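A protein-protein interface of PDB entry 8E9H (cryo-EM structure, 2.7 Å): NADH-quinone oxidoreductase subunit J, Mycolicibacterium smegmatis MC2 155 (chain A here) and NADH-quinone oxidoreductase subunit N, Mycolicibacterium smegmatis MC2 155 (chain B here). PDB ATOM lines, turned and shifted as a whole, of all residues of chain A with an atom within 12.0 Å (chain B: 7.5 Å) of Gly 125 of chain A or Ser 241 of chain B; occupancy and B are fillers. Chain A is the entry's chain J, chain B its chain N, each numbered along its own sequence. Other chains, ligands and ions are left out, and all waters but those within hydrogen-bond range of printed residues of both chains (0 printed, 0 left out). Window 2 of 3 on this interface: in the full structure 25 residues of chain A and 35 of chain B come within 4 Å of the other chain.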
ATOM      1  N   ALA A 116      -0.958  -5.373  -5.750  1.00  0.00           N
ATOM      2  CA  ALA A 116      -1.981  -6.386  -5.532  1.00  0.00           C
ATOM      3  C   ALA A 116      -2.845  -6.032  -4.333  1.00  0.00           C
ATOM      4  O   ALA A 116      -4.076  -6.119  -4.392  1.00  0.00           O
ATOM      5  CB  ALA A 116      -1.329  -7.753  -5.341  1.00  0.00           C
ATOM      6  N   GLY A 117      -2.216  -5.622  -3.232  1.00  0.00           N
ATOM      7  CA  GLY A 117      -2.978  -5.268  -2.050  1.00  0.00           C
ATOM      8  C   GLY A 117      -3.884  -4.081  -2.288  1.00  0.00           C
ATOM      9  O   GLY A 117      -5.042  -4.071  -1.865  1.00  0.00           O
ATOM     10  N   PHE A 118      -3.372  -3.058  -2.972  1.00  0.00           N
ATOM     11  CA  PHE A 118      -4.188  -1.886  -3.250  1.00  0.00           C
ATOM     12  C   PHE A 118      -5.374  -2.246  -4.130  1.00  0.00           C
ATOM     13  O   PHE A 118      -6.500  -1.808  -3.878  1.00  0.00           O
ATOM     14  CB  PHE A 118      -3.350  -0.797  -3.910  1.00  0.00           C
ATOM     15  CG  PHE A 118      -4.151   0.395  -4.319  1.00  0.00           C
ATOM     16  CD1 PHE A 118      -4.501   1.357  -3.393  1.00  0.00           C
ATOM     17  CD2 PHE A 118      -4.573   0.544  -5.625  1.00  0.00           C
ATOM     18  CE1 PHE A 118      -5.248   2.447  -3.763  1.00  0.00           C
ATOM     19  CE2 PHE A 118      -5.320   1.634  -6.000  1.00  0.00           C
ATOM     20  CZ  PHE A 118      -5.661   2.585  -5.067  1.00  0.00           C
ATOM     21  N   GLY A 119      -5.142  -3.035  -5.178  1.00  0.00           N
ATOM     22  CA  GLY A 119      -6.244  -3.436  -6.033  1.00  0.00           C
ATOM     23  C   GLY A 119      -7.277  -4.256  -5.287  1.00  0.00           C
ATOM     24  O   GLY A 119      -8.483  -4.045  -5.441  1.00  0.00           O
ATOM     25  N   ILE A 120      -6.818  -5.195  -4.460  1.00  0.00           N
ATOM     26  CA  ILE A 120      -7.737  -6.024  -3.692  1.00  0.00           C
ATOM     27  C   ILE A 120      -8.566  -5.160  -2.756  1.00  0.00           C
ATOM     28  O   ILE A 120      -9.785  -5.325  -2.645  1.00  0.00           O
ATOM     29  CB  ILE A 120      -6.960  -7.104  -2.917  1.00  0.00           C
ATOM     30  CG1 ILE A 120      -6.362  -8.131  -3.881  1.00  0.00           C
ATOM     31  CG2 ILE A 120      -7.862  -7.782  -1.903  1.00  0.00           C
ATOM     32  CD1 ILE A 120      -7.384  -9.000  -4.582  1.00  0.00           C
ATOM     33  N   LEU A 121      -7.916  -4.225  -2.064  1.00  0.00           N
ATOM     34  CA  LEU A 121      -8.636  -3.374  -1.126  1.00  0.00           C
ATOM     35  C   LEU A 121      -9.622  -2.472  -1.849  1.00  0.00           C
ATOM     36  O   LEU A 121     -10.735  -2.245  -1.366  1.00  0.00           O
ATOM     37  CB  LEU A 121      -7.647  -2.548  -0.310  1.00  0.00           C
ATOM     38  CG  LEU A 121      -6.815  -3.371   0.671  1.00  0.00           C
ATOM     39  CD1 LEU A 121      -5.572  -2.613   1.089  1.00  0.00           C
ATOM     40  CD2 LEU A 121      -7.645  -3.745   1.880  1.00  0.00           C
ATOM     41  N   VAL A 122      -9.235  -1.946  -3.009  1.00  0.00           N
ATOM     42  CA  VAL A 122     -10.140  -1.095  -3.772  1.00  0.00           C
ATOM     43  C   VAL A 122     -11.365  -1.887  -4.200  1.00  0.00           C
ATOM     44  O   VAL A 122     -12.503  -1.416  -4.091  1.00  0.00           O
ATOM     45  CB  VAL A 122      -9.410  -0.488  -4.981  1.00  0.00           C
ATOM     46  CG1 VAL A 122     -10.404   0.073  -5.979  1.00  0.00           C
ATOM     47  CG2 VAL A 122      -8.451   0.588  -4.528  1.00  0.00           C
ATOM     48  N   ILE A 123     -11.151  -3.106  -4.693  1.00  0.00           N
ATOM     49  CA  ILE A 123     -12.276  -3.922  -5.133  1.00  0.00           C
ATOM     50  C   ILE A 123     -13.168  -4.275  -3.952  1.00  0.00           C
ATOM     51  O   ILE A 123     -14.400  -4.261  -4.060  1.00  0.00           O
ATOM     52  CB  ILE A 123     -11.770  -5.178  -5.863  1.00  0.00           C
ATOM     53  CG1 ILE A 123     -11.211  -4.787  -7.231  1.00  0.00           C
ATOM     54  CG2 ILE A 123     -12.890  -6.186  -6.017  1.00  0.00           C
ATOM     55  CD1 ILE A 123     -10.359  -5.850  -7.870  1.00  0.00           C
ATOM     56  N   ALA A 124     -12.567  -4.593  -2.806  1.00  0.00           N
ATOM     57  CA  ALA A 124     -13.358  -4.897  -1.620  1.00  0.00           C
ATOM     58  C   ALA A 124     -14.187  -3.695  -1.195  1.00  0.00           C
ATOM     59  O   ALA A 124     -15.363  -3.834  -0.842  1.00  0.00           O
ATOM     60  CB  ALA A 124     -12.445  -5.345  -0.482  1.00  0.00           C
ATOM     61  N   GLY A 125     -13.591  -2.503  -1.224  1.00  0.00           N
ATOM     62  CA  GLY A 125     -14.337  -1.304  -0.896  1.00  0.00           C
ATOM     63  C   GLY A 125     -15.474  -1.041  -1.857  1.00  0.00           C
ATOM     64  O   GLY A 125     -16.561  -0.632  -1.440  1.00  0.00           O
ATOM     65  N   ILE A 126     -15.249  -1.271  -3.151  1.00  0.00           N
ATOM     66  CA  ILE A 126     -16.318  -1.093  -4.125  1.00  0.00           C
ATOM     67  C   ILE A 126     -17.474  -2.032  -3.814  1.00  0.00           C
ATOM     68  O   ILE A 126     -18.636  -1.615  -3.750  1.00  0.00           O
ATOM     69  CB  ILE A 126     -15.787  -1.311  -5.552  1.00  0.00           C
ATOM     70  CG1 ILE A 126     -14.832  -0.183  -5.939  1.00  0.00           C
ATOM     71  CG2 ILE A 126     -16.939  -1.397  -6.535  1.00  0.00           C
ATOM     72  CD1 ILE A 126     -13.968  -0.498  -7.135  1.00  0.00           C
ATOM     73  N   GLY A 127     -17.172  -3.310  -3.603  1.00  0.00           N
ATOM     74  CA  GLY A 127     -18.223  -4.259  -3.287  1.00  0.00           C
ATOM     75  C   GLY A 127     -19.301  -4.247  -4.347  1.00  0.00           C
ATOM     76  O   GLY A 127     -19.033  -4.085  -5.542  1.00  0.00           O
ATOM     77  N   ASN A 128     -20.543  -4.415  -3.908  1.00  0.00           N
ATOM     78  CA  ASN A 128     -21.692  -4.370  -4.797  1.00  0.00           C
ATOM     79  C   ASN A 128     -22.379  -3.019  -4.662  1.00  0.00           C
ATOM     80  O   ASN A 128     -22.821  -2.651  -3.569  1.00  0.00           O
ATOM     81  CB  ASN A 128     -22.666  -5.500  -4.468  1.00  0.00           C
ATOM     82  CG  ASN A 128     -21.987  -6.850  -4.412  1.00  0.00           C
ATOM     83  OD1 ASN A 128     -21.250  -7.225  -5.322  1.00  0.00           O
ATOM     84  ND2 ASN A 128     -22.227  -7.588  -3.335  1.00  0.00           N
ATOM     85  N   VAL A 129     -22.465  -2.285  -5.769  1.00  0.00           N
ATOM     86  CA  VAL A 129     -23.023  -0.938  -5.742  1.00  0.00           C
ATOM     87  C   VAL A 129     -24.250  -0.865  -6.641  1.00  0.00           C
ATOM     88  O   VAL A 129     -25.279  -0.305  -6.251  1.00  0.00           O
ATOM     89  CB  VAL A 129     -21.971   0.107  -6.152  1.00  0.00           C
ATOM     90  CG1 VAL A 129     -21.495  -0.124  -7.569  1.00  0.00           C
ATOM     91  CG2 VAL A 129     -22.533   1.511  -5.999  1.00  0.00           C
ATOM     92  N   SER A 130     -24.158  -1.426  -7.846  1.00  0.00           N
ATOM     93  CA  SER A 130     -25.301  -1.395  -8.748  1.00  0.00           C
ATOM     94  C   SER A 130     -26.506  -2.119  -8.175  1.00  0.00           C
ATOM     95  O   SER A 130     -27.629  -1.873  -8.629  1.00  0.00           O
ATOM     96  CB  SER A 130     -24.931  -2.006 -10.097  1.00  0.00           C
ATOM     97  OG  SER A 130     -24.476  -3.336  -9.941  1.00  0.00           O
ATOM     98  N   VAL A 131     -26.309  -2.999  -7.192  1.00  0.00           N
ATOM     99  CA  VAL A 131     -27.438  -3.640  -6.533  1.00  0.00           C
ATOM    100  C   VAL A 131     -28.350  -2.607  -5.897  1.00  0.00           C
ATOM    101  O   VAL A 131     -29.547  -2.857  -5.729  1.00  0.00           O
ATOM    102  CB  VAL A 131     -26.941  -4.649  -5.480  1.00  0.00           C
ATOM    103  CG1 VAL A 131     -26.273  -3.924  -4.324  1.00  0.00           C
ATOM    104  CG2 VAL A 131     -28.092  -5.508  -4.986  1.00  0.00           C
ATOM    105  N   ALA A 132     -27.812  -1.443  -5.541  1.00  0.00           N
ATOM    106  CA  ALA A 132     -28.587  -0.374  -4.931  1.00  0.00           C
ATOM    107  C   ALA A 132     -29.328   0.477  -5.952  1.00  0.00           C
ATOM    108  O   ALA A 132     -29.699   1.612  -5.635  1.00  0.00           O
ATOM    109  CB  ALA A 132     -27.674   0.514  -4.086  1.00  0.00           C
ATOM    110  N   MET B 216     -14.944   7.740  -6.856  1.00  0.00           N
ATOM    111  CA  MET B 216     -15.610   6.914  -5.856  1.00  0.00           C
ATOM    112  C   MET B 216     -16.641   7.720  -5.075  1.00  0.00           C
ATOM    113  O   MET B 216     -17.748   7.235  -4.818  1.00  0.00           O
ATOM    114  CB  MET B 216     -14.575   6.306  -4.912  1.00  0.00           C
ATOM    115  CG  MET B 216     -13.741   5.181  -5.512  1.00  0.00           C
ATOM    116  SD  MET B 216     -14.652   4.043  -6.572  1.00  0.00           S
ATOM    117  CE  MET B 216     -13.364   3.532  -7.700  1.00  0.00           C
ATOM    118  N   SER B 220     -20.657   7.075  -4.847  1.00  0.00           N
ATOM    119  CA  SER B 220     -21.369   6.890  -3.589  1.00  0.00           C
ATOM    120  C   SER B 220     -22.507   7.887  -3.438  1.00  0.00           C
ATOM    121  O   SER B 220     -23.602   7.512  -3.008  1.00  0.00           O
ATOM    122  CB  SER B 220     -20.405   7.024  -2.416  1.00  0.00           C
ATOM    123  OG  SER B 220     -20.218   8.384  -2.077  1.00  0.00           O
ATOM    124  N   GLY B 238     -26.182   7.243   0.222  1.00  0.00           N
ATOM    125  CA  GLY B 238     -25.052   6.747  -0.530  1.00  0.00           C
ATOM    126  C   GLY B 238     -24.707   5.310  -0.193  1.00  0.00           C
ATOM    127  O   GLY B 238     -25.351   4.642   0.617  1.00  0.00           O
ATOM    128  N   ASN B 239     -23.655   4.826  -0.853  1.00  0.00           N
ATOM    129  CA  ASN B 239     -23.199   3.459  -0.646  1.00  0.00           C
ATOM    130  C   ASN B 239     -22.495   3.276   0.692  1.00  0.00           C
ATOM    131  O   ASN B 239     -22.607   2.204   1.295  1.00  0.00           O
ATOM    132  CB  ASN B 239     -22.274   3.050  -1.788  1.00  0.00           C
ATOM    133  CG  ASN B 239     -21.464   1.823  -1.466  1.00  0.00           C
ATOM    134  OD1 ASN B 239     -20.420   1.910  -0.825  1.00  0.00           O
ATOM    135  ND2 ASN B 239     -21.935   0.667  -1.913  1.00  0.00           N
ATOM    136  N   THR B 240     -21.763   4.288   1.161  1.00  0.00           N
ATOM    137  CA  THR B 240     -21.111   4.264   2.468  1.00  0.00           C
ATOM    138  C   THR B 240     -19.871   3.382   2.480  1.00  0.00           C
ATOM    139  O   THR B 240     -19.139   3.353   3.473  1.00  0.00           O
ATOM    140  CB  THR B 240     -22.079   3.789   3.555  1.00  0.00           C
ATOM    141  OG1 THR B 240     -22.379   2.401   3.364  1.00  0.00           O
ATOM    142  CG2 THR B 240     -23.367   4.598   3.522  1.00  0.00           C
ATOM    143  N   SER B 241     -19.626   2.654   1.392  1.00  0.00           N
ATOM    144  CA  SER B 241     -18.330   2.007   1.212  1.00  0.00           C
ATOM    145  C   SER B 241     -17.547   2.711   0.119  1.00  0.00           C
ATOM    146  O   SER B 241     -16.347   2.973   0.261  1.00  0.00           O
ATOM    147  CB  SER B 241     -18.514   0.528   0.883  1.00  0.00           C
ATOM    148  OG  SER B 241     -19.457  -0.071   1.751  1.00  0.00           O
ATOM    149  N   LEU B 242     -18.221   3.039  -0.984  1.00  0.00           N
ATOM    150  CA  LEU B 242     -17.615   3.912  -1.976  1.00  0.00           C
ATOM    151  C   LEU B 242     -17.283   5.265  -1.379  1.00  0.00           C
ATOM    152  O   LEU B 242     -16.265   5.861  -1.732  1.00  0.00           O
ATOM    153  CB  LEU B 242     -18.547   4.086  -3.170  1.00  0.00           C
ATOM    154  CG  LEU B 242     -18.681   2.885  -4.097  1.00  0.00           C
ATOM    155  CD1 LEU B 242     -19.722   3.170  -5.148  1.00  0.00           C
ATOM    156  CD2 LEU B 242     -17.354   2.556  -4.742  1.00  0.00           C
ATOM    157  N   ALA B 243     -18.123   5.771  -0.477  1.00  0.00           N
ATOM    158  CA  ALA B 243     -17.809   7.040   0.164  1.00  0.00           C
ATOM    159  C   ALA B 243     -16.497   6.956   0.926  1.00  0.00           C
ATOM    160  O   ALA B 243     -15.639   7.832   0.793  1.00  0.00           O
ATOM    161  CB  ALA B 243     -18.944   7.451   1.099  1.00  0.00           C
ATOM    162  N   LEU B 244     -16.312   5.897   1.715  1.00  0.00           N
ATOM    163  CA  LEU B 244     -15.080   5.756   2.483  1.00  0.00           C
ATOM    164  C   LEU B 244     -13.883   5.554   1.567  1.00  0.00           C
ATOM    165  O   LEU B 244     -12.813   6.131   1.790  1.00  0.00           O
ATOM    166  CB  LEU B 244     -15.206   4.592   3.463  1.00  0.00           C
ATOM    167  CG  LEU B 244     -16.242   4.781   4.567  1.00  0.00           C
ATOM    168  CD1 LEU B 244     -16.432   3.488   5.335  1.00  0.00           C
ATOM    169  CD2 LEU B 244     -15.833   5.902   5.499  1.00  0.00           C
ATOM    170  N   LEU B 245     -14.039   4.729   0.533  1.00  0.00           N
ATOM    171  CA  LEU B 245     -12.932   4.496  -0.386  1.00  0.00           C
ATOM    172  C   LEU B 245     -12.533   5.783  -1.094  1.00  0.00           C
ATOM    173  O   LEU B 245     -11.342   6.079  -1.244  1.00  0.00           O
ATOM    174  CB  LEU B 245     -13.319   3.422  -1.398  1.00  0.00           C
ATOM    175  CG  LEU B 245     -12.307   3.144  -2.504  1.00  0.00           C
ATOM    176  CD1 LEU B 245     -11.015   2.622  -1.914  1.00  0.00           C
ATOM    177  CD2 LEU B 245     -12.882   2.156  -3.495  1.00  0.00           C
ATOM    178  N   GLY B 246     -13.517   6.563  -1.537  1.00  0.00           N
ATOM    179  CA  GLY B 246     -13.214   7.829  -2.170  1.00  0.00           C
ATOM    180  C   GLY B 246     -12.575   8.810  -1.213  1.00  0.00           C
ATOM    181  O   GLY B 246     -11.667   9.551  -1.587  1.00  0.00           O
ATOM    182  N   VAL B 247     -13.038   8.831   0.035  1.00  0.00           N
ATOM    183  CA  VAL B 247     -12.409   9.692   1.028  1.00  0.00           C
ATOM    184  C   VAL B 247     -10.948   9.312   1.186  1.00  0.00           C
ATOM    185  O   VAL B 247     -10.069  10.175   1.232  1.00  0.00           O
ATOM    186  CB  VAL B 247     -13.158   9.610   2.368  1.00  0.00           C
ATOM    187  CG1 VAL B 247     -12.283  10.137   3.489  1.00  0.00           C
ATOM    188  CG2 VAL B 247     -14.448  10.395   2.296  1.00  0.00           C
ATOM    189  N   LEU B 305     -18.801  11.168   8.334  1.00  0.00           N
ATOM    190  CA  LEU B 305     -17.968   9.985   8.479  1.00  0.00           C
ATOM    191  C   LEU B 305     -16.761  10.235   9.369  1.00  0.00           C
ATOM    192  O   LEU B 305     -15.731   9.575   9.207  1.00  0.00           O
ATOM    193  CB  LEU B 305     -17.513   9.485   7.109  1.00  0.00           C
ATOM    194  CG  LEU B 305     -18.610   9.357   6.055  1.00  0.00           C
ATOM    195  CD1 LEU B 305     -18.051   8.761   4.780  1.00  0.00           C
ATOM    196  CD2 LEU B 305     -19.754   8.509   6.579  1.00  0.00           C
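O of Ser 220 of chain B sits at hydrogen-bond distance from N of Asn 239 of chain B, 3.4 Å away.
OD1 of Asn 239 of chain B sits at hydrogen-bond distance from N of Ser 241 of chain B.
The side-chain amide oxygen (OD1) of Asn 239 of chain B lies within hydrogen-bond range of the backbone NH (N) of Leu 242 of chain B, 2.5 Å away.
Among the printed residues, pairs that only touch across the chains: Gly 125 of chain A with Ser 241 of chain B, Val 129 of chain A with Leu 242 of chain B, Val 122 of chain A with Leu 245 of chain B, Asn 128 of chain A with Asn 239 of chain B, Ile 126 of chain A with Leu 242 of chain B and Ile 126 of chain A with Leu 245 of chain B.
Of the 17 printed residues of chain A, 5 touch a printed residue of chain B.
Printed residues of chain A that touch a printed residue of chain B: Val 122, Gly 125, Ile 126, Asn 128 and Val 129.
Among the printed residues, 6 pairs touch across the chains.
Among the printed residues, no Asp or Glu carboxylate lies within 4 Å of a Lys or Arg side-chain nitrogen of the other chain.
Printed residues of chain B within 4 Å of Val 122 of chain A: Leu 245 (3.6 Å).
No residue of chain B comes within 4 Å of Ala 124 of chain A.
Of the printed residues of chain B, Gly 125 of chain A touches Ser 241.
Printed residues of chain B within 4 Å of Asn 128 of chain A: Asn 239 (3.8 Å).
Of the printed residues of chain B, Val 129 of chain A touches Leu 242 (3.4 Å).
No residue of chain A comes within 4 Å of Ser 220 of chain B.
Asn 239 of chain B touches one residue of chain A.
No residue of chain A comes within 4 Å of Thr 240 of chain B.
Of the printed residues of chain A, Ser 241 of chain B touches Gly 125 (3.2 Å).
Leu 242 of chain B touches just these residues of chain A: Ile 126 (3.8 Å) and Val 129 (3.4 Å).
No residue of chain A comes within 4 Å of Ala 243 of chain B.
The nearest residue of chain B that does not touch Gly 125 of chain A is Leu 242 of chain B (4.1 Å).
The nearest residue of chain A that does not touch Ser 241 of chain B is Ile 126 of chain A (5.1 Å).
The nearest printed residue of chain B that does not touch Val 129 of chain A is Asn 239 of chain B (4.2 Å).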
